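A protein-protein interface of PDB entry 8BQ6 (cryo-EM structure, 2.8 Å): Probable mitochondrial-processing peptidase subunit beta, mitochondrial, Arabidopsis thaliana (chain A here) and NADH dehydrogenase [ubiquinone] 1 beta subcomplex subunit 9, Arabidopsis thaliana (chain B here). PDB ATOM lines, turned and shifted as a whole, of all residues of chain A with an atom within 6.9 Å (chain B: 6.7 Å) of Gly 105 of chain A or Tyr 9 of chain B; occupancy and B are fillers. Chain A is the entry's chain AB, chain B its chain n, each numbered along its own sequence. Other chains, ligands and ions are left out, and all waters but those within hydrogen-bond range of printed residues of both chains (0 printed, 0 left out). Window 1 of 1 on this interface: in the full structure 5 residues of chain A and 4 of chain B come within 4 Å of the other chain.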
ATOM      1  N   THR A 100     -18.797   7.408  -7.734  1.00  0.00           N
ATOM      2  CA  THR A 100     -17.768   7.463  -8.759  1.00  0.00           C
ATOM      3  C   THR A 100     -17.982   8.706  -9.606  1.00  0.00           C
ATOM      4  O   THR A 100     -19.121   9.131  -9.822  1.00  0.00           O
ATOM      5  CB  THR A 100     -17.761   6.202  -9.635  1.00  0.00           C
ATOM      6  OG1 THR A 100     -16.491   6.088 -10.289  1.00  0.00           O
ATOM      7  CG2 THR A 100     -18.834   6.261 -10.689  1.00  0.00           C
ATOM      8  N   THR A 101     -16.884   9.305 -10.042  1.00  0.00           N
ATOM      9  CA  THR A 101     -16.920  10.452 -10.931  1.00  0.00           C
ATOM     10  C   THR A 101     -16.395  10.033 -12.293  1.00  0.00           C
ATOM     11  O   THR A 101     -15.267   9.544 -12.409  1.00  0.00           O
ATOM     12  CB  THR A 101     -16.095  11.606 -10.362  1.00  0.00           C
ATOM     13  OG1 THR A 101     -16.323  11.693  -8.951  1.00  0.00           O
ATOM     14  CG2 THR A 101     -16.487  12.921 -11.014  1.00  0.00           C
ATOM     15  N   LEU A 102     -17.221  10.210 -13.315  1.00  0.00           N
ATOM     16  CA  LEU A 102     -16.840   9.883 -14.670  1.00  0.00           C
ATOM     17  C   LEU A 102     -15.812  10.899 -15.153  1.00  0.00           C
ATOM     18  O   LEU A 102     -15.660  11.969 -14.562  1.00  0.00           O
ATOM     19  CB  LEU A 102     -18.079   9.860 -15.562  1.00  0.00           C
ATOM     20  CG  LEU A 102     -19.033   8.694 -15.309  1.00  0.00           C
ATOM     21  CD1 LEU A 102     -19.829   8.374 -16.554  1.00  0.00           C
ATOM     22  CD2 LEU A 102     -18.251   7.478 -14.855  1.00  0.00           C
ATOM     23  N   PRO A 103     -15.064  10.581 -16.215  1.00  0.00           N
ATOM     24  CA  PRO A 103     -14.053  11.537 -16.693  1.00  0.00           C
ATOM     25  C   PRO A 103     -14.630  12.885 -17.080  1.00  0.00           C
ATOM     26  O   PRO A 103     -13.914  13.891 -17.015  1.00  0.00           O
ATOM     27  CB  PRO A 103     -13.436  10.821 -17.901  1.00  0.00           C
ATOM     28  CG  PRO A 103     -13.718   9.387 -17.674  1.00  0.00           C
ATOM     29  CD  PRO A 103     -15.044   9.333 -16.997  1.00  0.00           C
ATOM     30  N   ASN A 104     -15.899  12.939 -17.473  1.00  0.00           N
ATOM     31  CA  ASN A 104     -16.534  14.173 -17.913  1.00  0.00           C
ATOM     32  C   ASN A 104     -17.209  14.941 -16.783  1.00  0.00           C
ATOM     33  O   ASN A 104     -17.832  15.975 -17.044  1.00  0.00           O
ATOM     34  CB  ASN A 104     -17.570  13.882 -18.994  1.00  0.00           C
ATOM     35  CG  ASN A 104     -18.614  12.902 -18.533  1.00  0.00           C
ATOM     36  OD1 ASN A 104     -18.497  12.321 -17.457  1.00  0.00           O
ATOM     37  ND2 ASN A 104     -19.667  12.745 -19.317  1.00  0.00           N
ATOM     38  N   GLY A 105     -17.127  14.455 -15.546  1.00  0.00           N
ATOM     39  CA  GLY A 105     -17.703  15.139 -14.407  1.00  0.00           C
ATOM     40  C   GLY A 105     -18.963  14.516 -13.845  1.00  0.00           C
ATOM     41  O   GLY A 105     -19.325  14.824 -12.702  1.00  0.00           O
ATOM     42  N   LEU A 106     -19.633  13.652 -14.601  1.00  0.00           N
ATOM     43  CA  LEU A 106     -20.831  12.990 -14.107  1.00  0.00           C
ATOM     44  C   LEU A 106     -20.514  12.133 -12.888  1.00  0.00           C
ATOM     45  O   LEU A 106     -19.461  11.497 -12.811  1.00  0.00           O
ATOM     46  CB  LEU A 106     -21.434  12.131 -15.214  1.00  0.00           C
ATOM     47  CG  LEU A 106     -22.914  11.793 -15.107  1.00  0.00           C
ATOM     48  CD1 LEU A 106     -23.697  13.053 -14.881  1.00  0.00           C
ATOM     49  CD2 LEU A 106     -23.368  11.119 -16.379  1.00  0.00           C
ATOM     50  N   ARG A 107     -21.433  12.119 -11.928  1.00  0.00           N
ATOM     51  CA  ARG A 107     -21.290  11.324 -10.716  1.00  0.00           C
ATOM     52  C   ARG A 107     -22.314  10.202 -10.724  1.00  0.00           C
ATOM     53  O   ARG A 107     -23.459  10.401 -11.142  1.00  0.00           O
ATOM     54  CB  ARG A 107     -21.449  12.188  -9.465  1.00  0.00           C
ATOM     55  CG  ARG A 107     -20.235  13.050  -9.176  1.00  0.00           C
ATOM     56  CD  ARG A 107     -20.482  14.055  -8.065  1.00  0.00           C
ATOM     57  NE  ARG A 107     -21.124  15.259  -8.573  1.00  0.00           N
ATOM     58  CZ  ARG A 107     -21.644  16.216  -7.815  1.00  0.00           C
ATOM     59  NH1 ARG A 107     -21.581  16.162  -6.495  1.00  0.00           N
ATOM     60  NH2 ARG A 107     -22.229  17.257  -8.397  1.00  0.00           N
ATOM     61  N   VAL A 108     -21.893   9.021 -10.289  1.00  0.00           N
ATOM     62  CA  VAL A 108     -22.773   7.870 -10.146  1.00  0.00           C
ATOM     63  C   VAL A 108     -22.690   7.404  -8.703  1.00  0.00           C
ATOM     64  O   VAL A 108     -21.602   7.078  -8.212  1.00  0.00           O
ATOM     65  CB  VAL A 108     -22.401   6.739 -11.115  1.00  0.00           C
ATOM     66  CG1 VAL A 108     -23.461   5.674 -11.092  1.00  0.00           C
ATOM     67  CG2 VAL A 108     -22.228   7.282 -12.525  1.00  0.00           C
ATOM     68  N   ALA A 276     -22.831  17.673 -17.520  1.00  0.00           N
ATOM     69  CA  ALA A 276     -22.357  16.526 -16.750  1.00  0.00           C
ATOM     70  C   ALA A 276     -21.961  16.917 -15.334  1.00  0.00           C
ATOM     71  O   ALA A 276     -22.266  16.195 -14.377  1.00  0.00           O
ATOM     72  CB  ALA A 276     -21.174  15.867 -17.459  1.00  0.00           C
ATOM     73  N   SER A 277     -21.281  18.049 -15.174  1.00  0.00           N
ATOM     74  CA  SER A 277     -20.785  18.419 -13.857  1.00  0.00           C
ATOM     75  C   SER A 277     -21.895  18.819 -12.898  1.00  0.00           C
ATOM     76  O   SER A 277     -21.634  18.951 -11.698  1.00  0.00           O
ATOM     77  CB  SER A 277     -19.770  19.552 -13.985  1.00  0.00           C
ATOM     78  OG  SER A 277     -19.330  19.985 -12.713  1.00  0.00           O
ATOM     79  N   ARG A 278     -23.118  19.008 -13.394  1.00  0.00           N
ATOM     80  CA  ARG A 278     -24.256  19.429 -12.590  1.00  0.00           C
ATOM     81  C   ARG A 278     -25.255  18.307 -12.343  1.00  0.00           C
ATOM     82  O   ARG A 278     -26.232  18.509 -11.614  1.00  0.00           O
ATOM     83  CB  ARG A 278     -24.957  20.608 -13.264  1.00  0.00           C
ATOM     84  CG  ARG A 278     -24.197  21.915 -13.149  1.00  0.00           C
ATOM     85  CD  ARG A 278     -24.808  23.004 -14.013  1.00  0.00           C
ATOM     86  NE  ARG A 278     -26.079  23.479 -13.481  1.00  0.00           N
ATOM     87  CZ  ARG A 278     -26.755  24.510 -13.968  1.00  0.00           C
ATOM     88  NH1 ARG A 278     -26.300  25.216 -14.989  1.00  0.00           N
ATOM     89  NH2 ARG A 278     -27.917  24.843 -13.412  1.00  0.00           N
ATOM     90  N   MET A 279     -25.032  17.130 -12.921  1.00  0.00           N
ATOM     91  CA  MET A 279     -25.968  16.020 -12.842  1.00  0.00           C
ATOM     92  C   MET A 279     -25.385  14.897 -12.000  1.00  0.00           C
ATOM     93  O   MET A 279     -24.171  14.670 -12.001  1.00  0.00           O
ATOM     94  CB  MET A 279     -26.321  15.499 -14.238  1.00  0.00           C
ATOM     95  CG  MET A 279     -26.916  16.552 -15.154  1.00  0.00           C
ATOM     96  SD  MET A 279     -27.420  15.932 -16.771  1.00  0.00           S
ATOM     97  CE  MET A 279     -27.496  14.170 -16.471  1.00  0.00           C
ATOM     98  N   VAL A 280     -26.258  14.206 -11.275  1.00  0.00           N
ATOM     99  CA  VAL A 280     -25.893  13.049 -10.469  1.00  0.00           C
ATOM    100  C   VAL A 280     -26.882  11.935 -10.773  1.00  0.00           C
ATOM    101  O   VAL A 280     -28.093  12.177 -10.841  1.00  0.00           O
ATOM    102  CB  VAL A 280     -25.882  13.389  -8.968  1.00  0.00           C
ATOM    103  CG1 VAL A 280     -25.912  12.129  -8.125  1.00  0.00           C
ATOM    104  CG2 VAL A 280     -24.654  14.207  -8.636  1.00  0.00           C
ATOM    105  N   SER A 305     -21.753  19.717 -21.703  1.00  0.00           N
ATOM    106  CA  SER A 305     -20.419  20.163 -21.289  1.00  0.00           C
ATOM    107  C   SER A 305     -20.272  21.679 -21.384  1.00  0.00           C
ATOM    108  O   SER A 305     -19.211  22.198 -21.741  1.00  0.00           O
ATOM    109  CB  SER A 305     -19.321  19.462 -22.090  1.00  0.00           C
ATOM    110  OG  SER A 305     -19.401  18.062 -21.894  1.00  0.00           O
ATOM    111  N   ALA B   7     -11.283  18.851 -24.029  1.00  0.00           N
ATOM    112  CA  ALA B   7     -12.528  18.935 -23.279  1.00  0.00           C
ATOM    113  C   ALA B   7     -12.524  20.156 -22.370  1.00  0.00           C
ATOM    114  O   ALA B   7     -11.708  21.062 -22.529  1.00  0.00           O
ATOM    115  CB  ALA B   7     -12.748  17.668 -22.467  1.00  0.00           C
ATOM    116  N   ALA B   8     -13.451  20.177 -21.424  1.00  0.00           N
ATOM    117  CA  ALA B   8     -13.558  21.253 -20.451  1.00  0.00           C
ATOM    118  C   ALA B   8     -13.250  20.800 -19.037  1.00  0.00           C
ATOM    119  O   ALA B   8     -12.599  21.530 -18.287  1.00  0.00           O
ATOM    120  CB  ALA B   8     -14.963  21.865 -20.494  1.00  0.00           C
ATOM    121  N   TYR B   9     -13.712  19.610 -18.655  1.00  0.00           N
ATOM    122  CA  TYR B   9     -13.364  19.067 -17.351  1.00  0.00           C
ATOM    123  C   TYR B   9     -11.869  18.819 -17.235  1.00  0.00           C
ATOM    124  O   TYR B   9     -11.297  18.990 -16.155  1.00  0.00           O
ATOM    125  CB  TYR B   9     -14.141  17.780 -17.102  1.00  0.00           C
ATOM    126  CG  TYR B   9     -14.125  17.350 -15.669  1.00  0.00           C
ATOM    127  CD1 TYR B   9     -14.967  17.950 -14.754  1.00  0.00           C
ATOM    128  CD2 TYR B   9     -13.290  16.336 -15.231  1.00  0.00           C
ATOM    129  CE1 TYR B   9     -14.971  17.573 -13.447  1.00  0.00           C
ATOM    130  CE2 TYR B   9     -13.291  15.944 -13.914  1.00  0.00           C
ATOM    131  CZ  TYR B   9     -14.137  16.572 -13.027  1.00  0.00           C
ATOM    132  OH  TYR B   9     -14.162  16.211 -11.710  1.00  0.00           O
ATOM    133  N   PHE B  10     -11.223  18.405 -18.327  1.00  0.00           N
ATOM    134  CA  PHE B  10      -9.768  18.303 -18.326  1.00  0.00           C
ATOM    135  C   PHE B  10      -9.133  19.664 -18.058  1.00  0.00           C
ATOM    136  O   PHE B  10      -8.352  19.806 -17.111  1.00  0.00           O
ATOM    137  CB  PHE B  10      -9.299  17.712 -19.663  1.00  0.00           C
ATOM    138  CG  PHE B  10      -7.789  17.612 -19.835  1.00  0.00           C
ATOM    139  CD1 PHE B  10      -7.046  16.586 -19.270  1.00  0.00           C
ATOM    140  CD2 PHE B  10      -7.111  18.596 -20.536  1.00  0.00           C
ATOM    141  CE1 PHE B  10      -5.673  16.533 -19.421  1.00  0.00           C
ATOM    142  CE2 PHE B  10      -5.739  18.546 -20.690  1.00  0.00           C
ATOM    143  CZ  PHE B  10      -5.021  17.514 -20.134  1.00  0.00           C
ATOM    144  N   ALA B  11      -9.480  20.688 -18.846  1.00  0.00           N
ATOM    145  CA  ALA B  11      -8.853  21.993 -18.644  1.00  0.00           C
ATOM    146  C   ALA B  11      -9.160  22.546 -17.258  1.00  0.00           C
ATOM    147  O   ALA B  11      -8.261  23.045 -16.572  1.00  0.00           O
ATOM    148  CB  ALA B  11      -9.301  22.978 -19.722  1.00  0.00           C
ATOM    149  N   ARG B  12     -10.421  22.448 -16.826  1.00  0.00           N
ATOM    150  CA  ARG B  12     -10.806  22.923 -15.501  1.00  0.00           C
ATOM    151  C   ARG B  12     -10.077  22.178 -14.393  1.00  0.00           C
ATOM    152  O   ARG B  12      -9.605  22.799 -13.434  1.00  0.00           O
ATOM    153  CB  ARG B  12     -12.319  22.790 -15.322  1.00  0.00           C
ATOM    154  CG  ARG B  12     -12.790  22.684 -13.882  1.00  0.00           C
ATOM    155  CD  ARG B  12     -14.071  23.484 -13.678  1.00  0.00           C
ATOM    156  NE  ARG B  12     -14.340  23.729 -12.267  1.00  0.00           N
ATOM    157  CZ  ARG B  12     -15.300  23.145 -11.563  1.00  0.00           C
ATOM    158  NH1 ARG B  12     -16.195  22.354 -12.132  1.00  0.00           N
ATOM    159  NH2 ARG B  12     -15.365  23.363 -10.253  1.00  0.00           N
ATOM    160  N   ARG B  13      -9.982  20.853 -14.487  1.00  0.00           N
ATOM    161  CA  ARG B  13      -9.232  20.138 -13.464  1.00  0.00           C
ATOM    162  C   ARG B  13      -7.736  20.360 -13.608  1.00  0.00           C
ATOM    163  O   ARG B  13      -7.047  20.510 -12.597  1.00  0.00           O
ATOM    164  CB  ARG B  13      -9.560  18.646 -13.492  1.00  0.00           C
ATOM    165  CG  ARG B  13     -10.934  18.335 -12.940  1.00  0.00           C
ATOM    166  CD  ARG B  13     -10.938  18.204 -11.419  1.00  0.00           C
ATOM    167  NE  ARG B  13     -10.007  17.190 -10.939  1.00  0.00           N
ATOM    168  CZ  ARG B  13      -8.968  17.426 -10.151  1.00  0.00           C
ATOM    169  NH1 ARG B  13      -8.700  18.640  -9.700  1.00  0.00           N
ATOM    170  NH2 ARG B  13      -8.182  16.414  -9.796  1.00  0.00           N
ATOM    171  N   ALA B  14      -7.223  20.411 -14.844  1.00  0.00           N
ATOM    172  CA  ALA B  14      -5.803  20.680 -15.048  1.00  0.00           C
ATOM    173  C   ALA B  14      -5.420  22.057 -14.530  1.00  0.00           C
ATOM    174  O   ALA B  14      -4.334  22.235 -13.966  1.00  0.00           O
ATOM    175  CB  ALA B  14      -5.433  20.552 -16.524  1.00  0.00           C
ATOM    176  N   ALA B  15      -6.284  23.052 -14.734  1.00  0.00           N
ATOM    177  CA  ALA B  15      -6.025  24.358 -14.140  1.00  0.00           C
ATOM    178  C   ALA B  15      -5.974  24.256 -12.626  1.00  0.00           C
ATOM    179  O   ALA B  15      -5.128  24.890 -11.986  1.00  0.00           O
ATOM    180  CB  ALA B  15      -7.088  25.362 -14.580  1.00  0.00           C
ATOM    181  N   GLN B  16      -6.857  23.446 -12.043  1.00  0.00           N
ATOM    182  CA  GLN B  16      -6.805  23.196 -10.608  1.00  0.00           C
ATOM    183  C   GLN B  16      -5.517  22.491 -10.216  1.00  0.00           C
ATOM    184  O   GLN B  16      -5.028  22.663  -9.094  1.00  0.00           O
ATOM    185  CB  GLN B  16      -8.005  22.360 -10.181  1.00  0.00           C
ATOM    186  CG  GLN B  16      -9.232  23.170  -9.887  1.00  0.00           C
ATOM    187  CD  GLN B  16     -10.415  22.306  -9.533  1.00  0.00           C
ATOM    188  OE1 GLN B  16     -10.598  21.225 -10.090  1.00  0.00           O
ATOM    189  NE2 GLN B  16     -11.231  22.779  -8.604  1.00  0.00           N
ATOM    190  N   GLU B  59     -12.308  13.976  -4.847  1.00  0.00           N
ATOM    191  CA  GLU B  59     -12.626  14.026  -6.300  1.00  0.00           C
ATOM    192  C   GLU B  59     -13.776  15.009  -6.565  1.00  0.00           C
ATOM    193  O   GLU B  59     -14.051  15.278  -7.750  1.00  0.00           O
ATOM    194  CB  GLU B  59     -12.956  12.627  -6.820  1.00  0.00           C
ATOM    195  CG  GLU B  59     -12.423  12.357  -8.219  1.00  0.00           C
ATOM    196  CD  GLU B  59     -11.085  13.000  -8.555  1.00  0.00           C
ATOM    197  OE1 GLU B  59     -10.047  12.478  -8.094  1.00  0.00           O
ATOM    198  OE2 GLU B  59     -11.082  14.017  -9.285  1.00  0.00           O
ATOM    199  N   ASP B  60     -14.412  15.524  -5.514  1.00  0.00           N
ATOM    200  CA  ASP B  60     -15.464  16.552  -5.717  1.00  0.00           C
ATOM    201  C   ASP B  60     -14.760  17.801  -6.241  1.00  0.00           C
ATOM    202  O   ASP B  60     -14.098  18.470  -5.436  1.00  0.00           O
ATOM    203  CB  ASP B  60     -16.272  16.812  -4.443  1.00  0.00           C
ATOM    204  CG  ASP B  60     -17.383  17.836  -4.619  1.00  0.00           C
ATOM    205  OD1 ASP B  60     -17.680  18.546  -3.644  1.00  0.00           O
ATOM    206  OD2 ASP B  60     -17.947  17.918  -5.733  1.00  0.00           O
ATOM    207  N   VAL B  61     -14.853  18.055  -7.546  1.00  0.00           N
ATOM    208  CA  VAL B  61     -14.168  19.208  -8.113  1.00  0.00           C
ATOM    209  C   VAL B  61     -14.460  20.468  -7.307  1.00  0.00           C
ATOM    210  O   VAL B  61     -13.611  21.360  -7.202  1.00  0.00           O
ATOM    211  CB  VAL B  61     -14.551  19.366  -9.596  1.00  0.00           C
ATOM    212  CG1 VAL B  61     -16.021  19.736  -9.747  1.00  0.00           C
ATOM    213  CG2 VAL B  61     -13.652  20.370 -10.277  1.00  0.00           C
ATOM    214  N   ILE B  64     -12.614  20.639  -3.962  1.00  0.00           N
ATOM    215  CA  ILE B  64     -11.180  20.907  -4.267  1.00  0.00           C
ATOM    216  C   ILE B  64     -11.002  22.420  -4.377  1.00  0.00           C
ATOM    217  O   ILE B  64     -10.101  22.941  -3.706  1.00  0.00           O
ATOM    218  CB  ILE B  64     -10.765  20.171  -5.557  1.00  0.00           C
ATOM    219  CG1 ILE B  64     -10.768  18.655  -5.366  1.00  0.00           C
ATOM    220  CG2 ILE B  64      -9.423  20.664  -6.076  1.00  0.00           C
ATOM    221  CD1 ILE B  64     -10.741  17.877  -6.657  1.00  0.00           C
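Of the printed residues of chain B, Pro 103 of chain A touches Tyr 9 (3.1 Å). Printed residues of chain B within 4 Å of Ser 277 of chain A: Arg 12 (3.97 Å). Leu 106 of chain A touches none of the printed residues of chain B. Thr 101 of chain A touches none of the printed residues of chain B. The nearest residue of chain B that does not touch Gly 105 of chain A is Val 61 of chain B (6.6 Å). The nearest printed residue of chain A that does not touch Tyr 9 of chain B is Asn 104 of chain A (4.1 Å). The nearest printed residue of chain A that does not touch Arg 12 of chain B is Gly 105 of chain A (7.7 Å).
Among the printed residues, merely in contact across the chains: Pro 103 of chain A with Tyr 9 of chain B, Gly 105 of chain A with Tyr 9 of chain B and Ser 277 of chain A with Arg 12 of chain B.
Printed residues of chain A that touch a printed residue of chain B: Pro 103, Gly 105 and Ser 277. Of the 14 printed residues of chain B, 2 touch a printed residue of chain A. Hydrophobic or aromatic side chains of chain B that line the printed part of chain A: Tyr 9. Among the printed residues, 3 pairs touch across the chains.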
